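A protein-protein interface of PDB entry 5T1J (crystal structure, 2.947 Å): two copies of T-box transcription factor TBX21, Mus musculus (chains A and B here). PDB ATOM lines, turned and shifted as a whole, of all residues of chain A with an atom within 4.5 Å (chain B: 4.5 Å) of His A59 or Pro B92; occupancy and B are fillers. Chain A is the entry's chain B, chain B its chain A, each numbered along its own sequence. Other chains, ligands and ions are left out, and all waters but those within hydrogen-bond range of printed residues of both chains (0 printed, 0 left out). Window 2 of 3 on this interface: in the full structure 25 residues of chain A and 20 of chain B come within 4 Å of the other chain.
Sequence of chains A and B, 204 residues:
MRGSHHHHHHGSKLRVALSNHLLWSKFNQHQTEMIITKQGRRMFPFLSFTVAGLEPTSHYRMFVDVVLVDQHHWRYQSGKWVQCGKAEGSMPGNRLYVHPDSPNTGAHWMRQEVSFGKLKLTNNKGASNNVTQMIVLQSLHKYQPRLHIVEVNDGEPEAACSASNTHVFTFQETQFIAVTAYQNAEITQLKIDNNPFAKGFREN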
ATOM      1  N   THR A  57       1.364   1.044  29.722  1.00  0.00           N
ATOM      2  CA  THR A  57       2.412   0.164  29.219  1.00  0.00           C
ATOM      3  C   THR A  57       2.183  -0.223  27.764  1.00  0.00           C
ATOM      4  O   THR A  57       2.911  -1.046  27.214  1.00  0.00           O
ATOM      5  CB  THR A  57       2.543  -1.101  30.076  1.00  0.00           C
ATOM      6  OG1 THR A  57       1.235  -1.638  30.312  1.00  0.00           O
ATOM      7  CG2 THR A  57       3.122  -0.731  31.429  1.00  0.00           C
ATOM      8  N   SER A  58       1.162   0.365  27.151  1.00  0.00           N
ATOM      9  CA  SER A  58       1.112   0.474  25.700  1.00  0.00           C
ATOM     10  C   SER A  58       2.087   1.600  25.369  1.00  0.00           C
ATOM     11  O   SER A  58       2.561   2.281  26.278  1.00  0.00           O
ATOM     12  CB  SER A  58      -0.303   0.771  25.188  1.00  0.00           C
ATOM     13  OG  SER A  58      -1.273  -0.054  25.811  1.00  0.00           O
ATOM     14  N   HIS A  59       2.435   1.788  24.103  1.00  0.00           N
ATOM     15  CA  HIS A  59       3.221   2.974  23.737  1.00  0.00           C
ATOM     16  C   HIS A  59       2.948   3.551  22.346  1.00  0.00           C
ATOM     17  O   HIS A  59       2.276   2.936  21.517  1.00  0.00           O
ATOM     18  CB  HIS A  59       4.725   2.702  23.912  1.00  0.00           C
ATOM     19  CG  HIS A  59       5.150   1.298  23.606  1.00  0.00           C
ATOM     20  ND1 HIS A  59       4.786   0.624  22.453  1.00  0.00           N
ATOM     21  CD2 HIS A  59       5.956   0.458  24.290  1.00  0.00           C
ATOM     22  CE1 HIS A  59       5.329  -0.579  22.465  1.00  0.00           C
ATOM     23  NE2 HIS A  59       6.043  -0.706  23.569  1.00  0.00           N
ATOM     24  N   TYR A  60       3.444   4.771  22.131  1.00  0.00           N
ATOM     25  CA  TYR A  60       2.956   5.640  21.055  1.00  0.00           C
ATOM     26  C   TYR A  60       4.016   6.501  20.340  1.00  0.00           C
ATOM     27  O   TYR A  60       5.098   6.761  20.870  1.00  0.00           O
ATOM     28  CB  TYR A  60       1.855   6.565  21.606  1.00  0.00           C
ATOM     29  CG  TYR A  60       0.816   5.890  22.495  1.00  0.00           C
ATOM     30  CD1 TYR A  60      -0.401   5.476  21.968  1.00  0.00           C
ATOM     31  CD2 TYR A  60       1.041   5.675  23.852  1.00  0.00           C
ATOM     32  CE1 TYR A  60      -1.364   4.868  22.757  1.00  0.00           C
ATOM     33  CE2 TYR A  60       0.078   5.054  24.650  1.00  0.00           C
ATOM     34  CZ  TYR A  60      -1.120   4.657  24.092  1.00  0.00           C
ATOM     35  OH  TYR A  60      -2.080   4.048  24.862  1.00  0.00           O
ATOM     36  N   ASN A 104       8.174   5.914  23.040  1.00  0.00           N
ATOM     37  CA  ASN A 104       8.449   5.656  24.437  1.00  0.00           C
ATOM     38  C   ASN A 104       7.111   5.360  25.123  1.00  0.00           C
ATOM     39  O   ASN A 104       6.057   5.631  24.546  1.00  0.00           O
ATOM     40  CB  ASN A 104       9.204   6.854  25.022  1.00  0.00           C
ATOM     41  CG  ASN A 104       9.719   6.596  26.395  1.00  0.00           C
ATOM     42  OD1 ASN A 104       9.049   5.980  27.214  1.00  0.00           O
ATOM     43  ND2 ASN A 104      10.964   7.001  26.638  1.00  0.00           N
ATOM     44  N   THR A 105       7.150   4.807  26.335  1.00  0.00           N
ATOM     45  CA  THR A 105       5.948   4.227  26.954  1.00  0.00           C
ATOM     46  C   THR A 105       4.800   5.218  27.006  1.00  0.00           C
ATOM     47  O   THR A 105       5.022   6.429  27.095  1.00  0.00           O
ATOM     48  CB  THR A 105       6.198   3.712  28.412  1.00  0.00           C
ATOM     49  OG1 THR A 105       5.858   4.735  29.363  1.00  0.00           O
ATOM     50  CG2 THR A 105       7.644   3.283  28.610  1.00  0.00           C
ATOM     51  N   GLY A 106       3.578   4.708  26.907  1.00  0.00           N
ATOM     52  CA  GLY A 106       2.422   5.558  27.062  1.00  0.00           C
ATOM     53  C   GLY A 106       2.504   6.297  28.378  1.00  0.00           C
ATOM     54  O   GLY A 106       2.332   7.522  28.438  1.00  0.00           O
ATOM     55  N   VAL A 152       0.845   2.500  17.948  1.00  0.00           N
ATOM     56  CA  VAL A 152       1.556   1.498  17.153  1.00  0.00           C
ATOM     57  C   VAL A 152       1.395   0.085  17.709  1.00  0.00           C
ATOM     58  O   VAL A 152       1.722  -0.204  18.865  1.00  0.00           O
ATOM     59  CB  VAL A 152       3.059   1.813  17.033  1.00  0.00           C
ATOM     60  CG1 VAL A 152       3.270   3.017  16.132  1.00  0.00           C
ATOM     61  CG2 VAL A 152       3.652   2.058  18.379  1.00  0.00           C
ATOM     62  N   ASN A 153       0.862  -0.782  16.858  1.00  0.00           N
ATOM     63  CA  ASN A 153       0.520  -2.149  17.221  1.00  0.00           C
ATOM     64  C   ASN A 153       1.566  -3.211  16.846  1.00  0.00           C
ATOM     65  O   ASN A 153       2.630  -2.899  16.307  1.00  0.00           O
ATOM     66  CB  ASN A 153      -0.816  -2.491  16.562  1.00  0.00           C
ATOM     67  CG  ASN A 153      -0.958  -1.849  15.187  1.00  0.00           C
ATOM     68  OD1 ASN A 153      -0.047  -1.166  14.717  1.00  0.00           O
ATOM     69  ND2 ASN A 153      -2.100  -2.058  14.544  1.00  0.00           N
ATOM     70  N   ASP A 154       1.249  -4.459  17.181  1.00  0.00           N
ATOM     71  CA  ASP A 154       1.969  -5.652  16.736  1.00  0.00           C
ATOM     72  C   ASP A 154       0.954  -6.656  16.219  1.00  0.00           C
ATOM     73  O   ASP A 154      -0.096  -6.850  16.833  1.00  0.00           O
ATOM     74  CB  ASP A 154       2.816  -6.243  17.865  1.00  0.00           C
ATOM     75  CG  ASP A 154       3.836  -5.253  18.389  1.00  0.00           C
ATOM     76  OD1 ASP A 154       4.898  -5.123  17.735  1.00  0.00           O
ATOM     77  OD2 ASP A 154       3.539  -4.541  19.383  1.00  0.00           O
ATOM     78  N   LEU B  68       8.828  -3.081  13.359  1.00  0.00           N
ATOM     79  CA  LEU B  68       9.396  -4.323  13.897  1.00  0.00           C
ATOM     80  C   LEU B  68       8.440  -5.526  13.845  1.00  0.00           C
ATOM     81  O   LEU B  68       7.368  -5.519  14.463  1.00  0.00           O
ATOM     82  CB  LEU B  68       9.840  -4.045  15.329  1.00  0.00           C
ATOM     83  CG  LEU B  68      10.548  -5.030  16.212  1.00  0.00           C
ATOM     84  CD1 LEU B  68      11.353  -4.226  17.198  1.00  0.00           C
ATOM     85  CD2 LEU B  68       9.480  -5.807  16.926  1.00  0.00           C
ATOM     86  N   GLN B  71       8.591  -9.174  18.572  1.00  0.00           N
ATOM     87  CA  GLN B  71       9.242  -8.906  19.853  1.00  0.00           C
ATOM     88  C   GLN B  71      10.588  -9.571  20.095  1.00  0.00           C
ATOM     89  O   GLN B  71      11.405  -9.060  20.877  1.00  0.00           O
ATOM     90  CB  GLN B  71       8.292  -9.282  20.995  1.00  0.00           C
ATOM     91  CG  GLN B  71       6.779  -9.199  20.674  1.00  0.00           C
ATOM     92  CD  GLN B  71       6.312  -7.860  20.075  1.00  0.00           C
ATOM     93  OE1 GLN B  71       6.921  -6.810  20.291  1.00  0.00           O
ATOM     94  NE2 GLN B  71       5.201  -7.902  19.344  1.00  0.00           N
ATOM     95  N   MET B  91      10.161  -1.286  21.679  1.00  0.00           N
ATOM     96  CA  MET B  91       8.919  -0.955  20.981  1.00  0.00           C
ATOM     97  C   MET B  91       8.242  -2.292  20.519  1.00  0.00           C
ATOM     98  O   MET B  91       8.286  -3.237  21.308  1.00  0.00           O
ATOM     99  CB  MET B  91       9.200   0.042  19.879  1.00  0.00           C
ATOM    100  CG  MET B  91       8.054   0.980  19.647  1.00  0.00           C
ATOM    101  SD  MET B  91       7.472   1.680  21.186  1.00  0.00           S
ATOM    102  CE  MET B  91       6.103   2.638  20.553  1.00  0.00           C
ATOM    103  N   PRO B  92       7.660  -2.446  19.284  1.00  0.00           N
ATOM    104  CA  PRO B  92       7.435  -2.145  17.837  1.00  0.00           C
ATOM    105  C   PRO B  92       8.290  -1.070  17.153  1.00  0.00           C
ATOM    106  O   PRO B  92       7.747  -0.098  16.610  1.00  0.00           O
ATOM    107  CB  PRO B  92       5.964  -1.710  17.790  1.00  0.00           C
ATOM    108  CG  PRO B  92       5.327  -2.321  18.967  1.00  0.00           C
ATOM    109  CD  PRO B  92       6.381  -2.820  19.922  1.00  0.00           C
ATOM    110  N   GLY B  93       9.607  -1.270  17.176  1.00  0.00           N
ATOM    111  CA  GLY B  93      10.592  -0.285  16.749  1.00  0.00           C
ATOM    112  C   GLY B  93      10.432   0.451  15.439  1.00  0.00           C
ATOM    113  O   GLY B  93       9.960  -0.127  14.444  1.00  0.00           O
ATOM    114  N   ASN B  94      10.868   1.714  15.435  1.00  0.00           N
ATOM    115  CA  ASN B  94      10.870   2.499  14.199  1.00  0.00           C
ATOM    116  C   ASN B  94      11.510   3.883  14.373  1.00  0.00           C
ATOM    117  O   ASN B  94      11.740   4.326  15.493  1.00  0.00           O
ATOM    118  CB  ASN B  94       9.430   2.679  13.703  1.00  0.00           C
ATOM    119  CG  ASN B  94       9.351   3.120  12.265  1.00  0.00           C
ATOM    120  OD1 ASN B  94       9.805   4.199  11.905  1.00  0.00           O
ATOM    121  ND2 ASN B  94       8.676   2.325  11.456  1.00  0.00           N
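Of chain B, only Met B91 and Pro B92 come within 4 Å of His A59.
Printed residues of chain B within 4 Å of Val A152: Met B91 (3.3 Å).
Printed residues of chain B within 4 Å of Asn A153: Pro B92 (3.8 Å).
Of the printed residues of chain A, Gln B71 touches Asp A154 (3.1 Å).
Of chain A, only His A59 (3.5 Å), Asn A153 (3.8 Å) and Asp A154 (2.9 Å) come within 4 Å of Pro B92.
Gly B93 touches none of the printed residues of chain A.
The nearest residue of chain A that does not touch Pro B92 is Val A152 (4.2 Å).
The nearest printed residue of chain A that does not touch Met B91 is Asn A104 (4.6 Å).
Among the printed residues, pairs that only touch across the chains: His A59 with Pro B92 (3.5 Å), Tyr A60 with Met B91 (3.8 Å), Val A152 with Met B91 (3.3 Å), Asn A153 with Pro B92 (3.8 Å) and Asp A154 with Pro B92 (2.9 Å).
Of the 6 printed residues of chain B, 3 touch a printed residue of chain A.
Printed residues of chain B that touch a printed residue of chain A: Gln B71, Met B91 and Pro B92.
Hydrophobic or aromatic side chains of chain B within 4 Å of the printed part of chain A: Met B91 and Pro B92.
Along chain A the printed residues that touch a printed residue of chain B span positions 59 to 154.
Among the printed residues, 7 pairs touch across the chains.
NE2 of Gln B71 sits close to OD1 of Asp A154, at 3.2 Å.
ND1 of His A59 sits close to SD of Met B91, at 3.2 Å.
No position is printed for both chains.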
